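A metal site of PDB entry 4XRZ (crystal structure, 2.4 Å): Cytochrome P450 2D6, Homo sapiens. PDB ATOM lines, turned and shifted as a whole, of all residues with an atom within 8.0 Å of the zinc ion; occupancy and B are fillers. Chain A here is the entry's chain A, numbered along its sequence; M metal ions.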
ATOM      1  N   ALA A 165      -6.393 -30.303 -16.326  1.00  0.00           N
ATOM      2  CA  ALA A 165      -5.735 -29.182 -15.667  1.00  0.00           C
ATOM      3  C   ALA A 165      -4.258 -29.164 -16.042  1.00  0.00           C
ATOM      4  O   ALA A 165      -3.656 -28.104 -16.211  1.00  0.00           O
ATOM      5  CB  ALA A 165      -5.899 -29.265 -14.157  1.00  0.00           C
ATOM      6  N   SER A 166      -3.677 -30.352 -16.189  1.00  0.00           N
ATOM      7  CA  SER A 166      -2.287 -30.482 -16.580  1.00  0.00           C
ATOM      8  C   SER A 166      -2.053 -29.995 -18.000  1.00  0.00           C
ATOM      9  O   SER A 166      -0.991 -29.448 -18.313  1.00  0.00           O
ATOM     10  CB  SER A 166      -1.836 -31.946 -16.450  1.00  0.00           C
ATOM     11  OG  SER A 166      -0.479 -32.096 -16.825  1.00  0.00           O
ATOM     12  N   LEU A 167      -3.043 -30.193 -18.860  1.00  0.00           N
ATOM     13  CA  LEU A 167      -2.948 -29.789 -20.259  1.00  0.00           C
ATOM     14  C   LEU A 167      -3.224 -28.300 -20.430  1.00  0.00           C
ATOM     15  O   LEU A 167      -2.618 -27.643 -21.276  1.00  0.00           O
ATOM     16  CB  LEU A 167      -3.906 -30.603 -21.117  1.00  0.00           C
ATOM     17  CG  LEU A 167      -3.505 -32.056 -21.382  1.00  0.00           C
ATOM     18  CD1 LEU A 167      -4.636 -32.807 -22.077  1.00  0.00           C
ATOM     19  CD2 LEU A 167      -2.239 -32.094 -22.217  1.00  0.00           C
ATOM     20  N   THR A 168      -4.150 -27.773 -19.635  1.00  0.00           N
ATOM     21  CA  THR A 168      -4.534 -26.368 -19.752  1.00  0.00           C
ATOM     22  C   THR A 168      -3.756 -25.458 -18.796  1.00  0.00           C
ATOM     23  O   THR A 168      -3.211 -24.437 -19.220  1.00  0.00           O
ATOM     24  CB  THR A 168      -6.044 -26.177 -19.486  1.00  0.00           C
ATOM     25  OG1 THR A 168      -6.341 -26.490 -18.121  1.00  0.00           O
ATOM     26  CG2 THR A 168      -6.855 -27.090 -20.401  1.00  0.00           C
ATOM     27  N   CYS A 169      -3.700 -25.821 -17.524  1.00  0.00           N
ATOM     28  CA  CYS A 169      -3.085 -24.976 -16.506  1.00  0.00           C
ATOM     29  C   CYS A 169      -1.616 -25.338 -16.268  1.00  0.00           C
ATOM     30  O   CYS A 169      -0.848 -24.555 -15.723  1.00  0.00           O
ATOM     31  CB  CYS A 169      -3.867 -25.058 -15.191  1.00  0.00           C
ATOM     32  SG  CYS A 169      -5.639 -24.644 -15.339  1.00  0.00           S
ATOM     33  N   GLY A 170      -1.220 -26.531 -16.714  1.00  0.00           N
ATOM     34  CA  GLY A 170       0.144 -26.978 -16.548  1.00  0.00           C
ATOM     35  C   GLY A 170       0.456 -27.468 -15.146  1.00  0.00           C
ATOM     36  O   GLY A 170       1.604 -27.421 -14.693  1.00  0.00           O
ATOM     37  N   ARG A 171      -0.568 -27.952 -14.442  1.00  0.00           N
ATOM     38  CA  ARG A 171      -0.394 -28.441 -13.087  1.00  0.00           C
ATOM     39  C   ARG A 171      -1.475 -29.430 -12.695  1.00  0.00           C
ATOM     40  O   ARG A 171      -2.508 -29.541 -13.358  1.00  0.00           O
ATOM     41  CB  ARG A 171      -0.374 -27.281 -12.085  1.00  0.00           C
ATOM     42  CG  ARG A 171      -1.748 -26.629 -11.904  1.00  0.00           C
ATOM     43  CD  ARG A 171      -1.803 -25.767 -10.655  1.00  0.00           C
ATOM     44  NE  ARG A 171      -1.617 -26.560  -9.434  1.00  0.00           N
ATOM     45  CZ  ARG A 171      -1.640 -26.058  -8.208  1.00  0.00           C
ATOM     46  NH1 ARG A 171      -1.835 -24.758  -8.016  1.00  0.00           N
ATOM     47  NH2 ARG A 171      -1.460 -26.864  -7.168  1.00  0.00           N
ATOM     48  N   HIS A 236      -1.247 -18.253 -12.682  1.00  0.00           N
ATOM     49  CA  HIS A 236      -0.559 -18.923 -13.778  1.00  0.00           C
ATOM     50  C   HIS A 236       0.220 -17.930 -14.627  1.00  0.00           C
ATOM     51  O   HIS A 236       1.315 -18.232 -15.098  1.00  0.00           O
ATOM     52  CB  HIS A 236      -1.559 -19.690 -14.637  1.00  0.00           C
ATOM     53  CG  HIS A 236      -0.927 -20.633 -15.613  1.00  0.00           C
ATOM     54  ND1 HIS A 236      -1.624 -21.247 -16.628  1.00  0.00           N
ATOM     55  CD2 HIS A 236       0.353 -21.063 -15.727  1.00  0.00           C
ATOM     56  CE1 HIS A 236      -0.809 -22.017 -17.325  1.00  0.00           C
ATOM     57  NE2 HIS A 236       0.399 -21.924 -16.795  1.00  0.00           N
ATOM     58  N   ARG A 237      -0.357 -16.738 -14.817  1.00  0.00           N
ATOM     59  CA  ARG A 237       0.296 -15.681 -15.578  1.00  0.00           C
ATOM     60  C   ARG A 237       1.646 -15.300 -14.968  1.00  0.00           C
ATOM     61  O   ARG A 237       2.616 -15.060 -15.683  1.00  0.00           O
ATOM     62  CB  ARG A 237      -0.591 -14.442 -15.646  1.00  0.00           C
ATOM     63  CG  ARG A 237      -1.456 -14.339 -16.891  1.00  0.00           C
ATOM     64  CD  ARG A 237      -1.979 -12.918 -17.063  1.00  0.00           C
ATOM     65  NE  ARG A 237      -2.844 -12.776 -18.238  1.00  0.00           N
ATOM     66  CZ  ARG A 237      -4.162 -12.906 -18.199  1.00  0.00           C
ATOM     67  NH1 ARG A 237      -4.777 -13.186 -17.060  1.00  0.00           N
ATOM     68  NH2 ARG A 237      -4.877 -12.761 -19.308  1.00  0.00           N
ATOM     69  N   THR A 239       3.695 -17.133 -13.216  1.00  0.00           N
ATOM     70  CA  THR A 239       4.696 -18.188 -13.332  1.00  0.00           C
ATOM     71  C   THR A 239       5.083 -18.491 -14.774  1.00  0.00           C
ATOM     72  O   THR A 239       6.066 -19.192 -15.029  1.00  0.00           O
ATOM     73  CB  THR A 239       4.217 -19.486 -12.663  1.00  0.00           C
ATOM     74  OG1 THR A 239       2.967 -19.889 -13.250  1.00  0.00           O
ATOM     75  CG2 THR A 239       4.036 -19.292 -11.169  1.00  0.00           C
ATOM     76  N   TRP A 240       4.317 -17.964 -15.723  1.00  0.00           N
ATOM     77  CA  TRP A 240       4.583 -18.187 -17.139  1.00  0.00           C
ATOM     78  C   TRP A 240       5.941 -17.640 -17.552  1.00  0.00           C
ATOM     79  O   TRP A 240       6.261 -16.482 -17.301  1.00  0.00           O
ATOM     80  CB  TRP A 240       3.486 -17.560 -18.004  1.00  0.00           C
ATOM     81  CG  TRP A 240       3.764 -17.636 -19.490  1.00  0.00           C
ATOM     82  CD1 TRP A 240       4.381 -18.649 -20.159  1.00  0.00           C
ATOM     83  CD2 TRP A 240       3.429 -16.644 -20.465  1.00  0.00           C
ATOM     84  NE1 TRP A 240       4.458 -18.355 -21.490  1.00  0.00           N
ATOM     85  CE2 TRP A 240       3.873 -17.128 -21.714  1.00  0.00           C
ATOM     86  CE3 TRP A 240       2.801 -15.399 -20.421  1.00  0.00           C
ATOM     87  CZ2 TRP A 240       3.716 -16.410 -22.893  1.00  0.00           C
ATOM     88  CZ3 TRP A 240       2.637 -14.687 -21.600  1.00  0.00           C
ATOM     89  CH2 TRP A 240       3.095 -15.200 -22.816  1.00  0.00           C
ATOM     90  N   ASP A 241       6.746 -18.484 -18.186  1.00  0.00           N
ATOM     91  CA  ASP A 241       8.029 -18.065 -18.739  1.00  0.00           C
ATOM     92  C   ASP A 241       7.951 -18.041 -20.260  1.00  0.00           C
ATOM     93  O   ASP A 241       8.101 -19.067 -20.913  1.00  0.00           O
ATOM     94  CB  ASP A 241       9.145 -19.004 -18.275  1.00  0.00           C
ATOM     95  CG  ASP A 241      10.529 -18.535 -18.709  1.00  0.00           C
ATOM     96  OD1 ASP A 241      11.487 -19.316 -18.584  1.00  0.00           O
ATOM     97  OD2 ASP A 241      10.651 -17.385 -19.176  1.00  0.00           O
ATOM     98  N   PRO A 245       9.299 -22.412 -24.668  1.00  0.00           N
ATOM     99  CA  PRO A 245       8.113 -22.888 -25.381  1.00  0.00           C
ATOM    100  C   PRO A 245       6.969 -23.173 -24.408  1.00  0.00           C
ATOM    101  O   PRO A 245       7.229 -23.651 -23.306  1.00  0.00           O
ATOM    102  CB  PRO A 245       8.586 -24.165 -26.063  1.00  0.00           C
ATOM    103  CG  PRO A 245      10.064 -23.999 -26.200  1.00  0.00           C
ATOM    104  CD  PRO A 245      10.488 -23.232 -24.979  1.00  0.00           C
ATOM    105  N   PRO A 246       5.722 -22.871 -24.811  1.00  0.00           N
ATOM    106  CA  PRO A 246       4.547 -23.090 -23.964  1.00  0.00           C
ATOM    107  C   PRO A 246       4.489 -24.500 -23.396  1.00  0.00           C
ATOM    108  O   PRO A 246       4.666 -25.474 -24.121  1.00  0.00           O
ATOM    109  CB  PRO A 246       3.363 -22.830 -24.907  1.00  0.00           C
ATOM    110  CG  PRO A 246       3.961 -22.788 -26.297  1.00  0.00           C
ATOM    111  CD  PRO A 246       5.361 -22.314 -26.114  1.00  0.00           C
ATOM    112  N   ARG A 247       4.241 -24.586 -22.085  1.00  0.00           N
ATOM    113  CA  ARG A 247       4.234 -25.858 -21.388  1.00  0.00           C
ATOM    114  C   ARG A 247       2.816 -26.418 -21.299  1.00  0.00           C
ATOM    115  O   ARG A 247       2.615 -27.580 -20.929  1.00  0.00           O
ATOM    116  CB  ARG A 247       4.814 -25.677 -19.982  1.00  0.00           C
ATOM    117  CG  ARG A 247       5.974 -26.605 -19.654  1.00  0.00           C
ATOM    118  CD  ARG A 247       6.423 -26.378 -18.226  1.00  0.00           C
ATOM    119  NE  ARG A 247       5.273 -26.179 -17.349  1.00  0.00           N
ATOM    120  CZ  ARG A 247       4.587 -27.159 -16.776  1.00  0.00           C
ATOM    121  NH1 ARG A 247       4.935 -28.422 -16.980  1.00  0.00           N
ATOM    122  NH2 ARG A 247       3.536 -26.873 -16.013  1.00  0.00           N
ATOM    123  N   ASP A 248       1.845 -25.586 -21.642  1.00  0.00           N
ATOM    124  CA  ASP A 248       0.438 -25.964 -21.575  1.00  0.00           C
ATOM    125  C   ASP A 248      -0.381 -25.067 -22.503  1.00  0.00           C
ATOM    126  O   ASP A 248       0.167 -24.183 -23.153  1.00  0.00           O
ATOM    127  CB  ASP A 248      -0.071 -25.856 -20.137  1.00  0.00           C
ATOM    128  CG  ASP A 248       0.309 -24.540 -19.484  1.00  0.00           C
ATOM    129  OD1 ASP A 248      -0.360 -23.527 -19.757  1.00  0.00           O
ATOM    130  OD2 ASP A 248       1.279 -24.524 -18.685  1.00  0.00           O
ATOM    131  N   LEU A 249      -1.687 -25.314 -22.552  1.00  0.00           N
ATOM    132  CA  LEU A 249      -2.548 -24.617 -23.508  1.00  0.00           C
ATOM    133  C   LEU A 249      -2.729 -23.134 -23.170  1.00  0.00           C
ATOM    134  O   LEU A 249      -2.815 -22.297 -24.061  1.00  0.00           O
ATOM    135  CB  LEU A 249      -3.918 -25.298 -23.591  1.00  0.00           C
ATOM    136  CG  LEU A 249      -4.860 -24.815 -24.692  1.00  0.00           C
ATOM    137  CD1 LEU A 249      -5.572 -25.981 -25.355  1.00  0.00           C
ATOM    138  CD2 LEU A 249      -5.877 -23.801 -24.169  1.00  0.00           C
ATOM    139  N   THR A 250      -2.787 -22.812 -21.874  1.00  0.00           N
ATOM    140  CA  THR A 250      -2.965 -21.430 -21.450  1.00  0.00           C
ATOM    141  C   THR A 250      -1.779 -20.564 -21.862  1.00  0.00           C
ATOM    142  O   THR A 250      -1.950 -19.442 -22.320  1.00  0.00           O
ATOM    143  CB  THR A 250      -3.166 -21.332 -19.928  1.00  0.00           C
ATOM    144  OG1 THR A 250      -4.340 -22.064 -19.557  1.00  0.00           O
ATOM    145  CG2 THR A 250      -3.333 -19.886 -19.505  1.00  0.00           C
ATOM    146  N   GLU A 251      -0.567 -21.097 -21.693  1.00  0.00           N
ATOM    147  CA  GLU A 251       0.637 -20.386 -22.087  1.00  0.00           C
ATOM    148  C   GLU A 251       0.676 -20.175 -23.592  1.00  0.00           C
ATOM    149  O   GLU A 251       1.119 -19.120 -24.077  1.00  0.00           O
ATOM    150  CB  GLU A 251       1.881 -21.136 -21.621  1.00  0.00           C
ATOM    151  CG  GLU A 251       2.036 -21.203 -20.108  1.00  0.00           C
ATOM    152  CD  GLU A 251       3.292 -21.940 -19.684  1.00  0.00           C
ATOM    153  OE1 GLU A 251       3.391 -22.301 -18.496  1.00  0.00           O
ATOM    154  OE2 GLU A 251       4.177 -22.152 -20.536  1.00  0.00           O
ATOM    155  N   ALA A 252       0.227 -21.180 -24.347  1.00  0.00           N
ATOM    156  CA  ALA A 252       0.179 -21.091 -25.800  1.00  0.00           C
ATOM    157  C   ALA A 252      -0.799 -20.002 -26.219  1.00  0.00           C
ATOM    158  O   ALA A 252      -0.541 -19.243 -27.153  1.00  0.00           O
ATOM    159  CB  ALA A 252      -0.218 -22.429 -26.400  1.00  0.00           C
ATOM    160  N   LEU A 254      -1.667 -17.389 -24.372  1.00  0.00           N
ATOM    161  CA  LEU A 254      -1.056 -16.121 -23.967  1.00  0.00           C
ATOM    162  C   LEU A 254      -0.025 -15.650 -24.991  1.00  0.00           C
ATOM    163  O   LEU A 254       0.074 -14.454 -25.285  1.00  0.00           O
ATOM    164  CB  LEU A 254      -0.408 -16.251 -22.596  1.00  0.00           C
ATOM    165  CG  LEU A 254      -1.333 -16.380 -21.389  1.00  0.00           C
ATOM    166  CD1 LEU A 254      -0.556 -16.859 -20.170  1.00  0.00           C
ATOM    167  CD2 LEU A 254      -2.027 -15.061 -21.093  1.00  0.00           C
HETATM  168 ZN    ZN M   1       1.911 -22.987 -17.458  1.00  0.00          ZN
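The zinc ion is bound by OE1 of Glu 251 (1.9 Å).
The zinc ion is bound by NE2 of His 236, 2.0 Å away.
The zinc ion is bound by OD2 of Asp 248 (2.1 Å).
Cys 169 touches the zinc ion.
Of the 21 residues printed, 4 come within 4 Å of the zinc ion.
The nearest printed residue that does not touch the zinc ion is Arg 247 (4.5 Å).
SG of Cys 169 lies within hydrogen-bond range of OG1 of Thr 168, 3.4 Å away.
O of Cys 169 sits close to NE2 of His 236 (3.1 Å).
The side-chain carboxylate of Asp 248 is in hydrogen-bond range of the backbone NH of Thr 250 (3.3 Å).
The backbone carbonyl oxygen (O) of His 236 sits at hydrogen-bond distance from the side-chain hydroxyl (OG1) of Thr 239, 3.0 Å away.
OE2 of Glu 251 lies within hydrogen-bond range of N of Arg 247 (2.9 Å).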
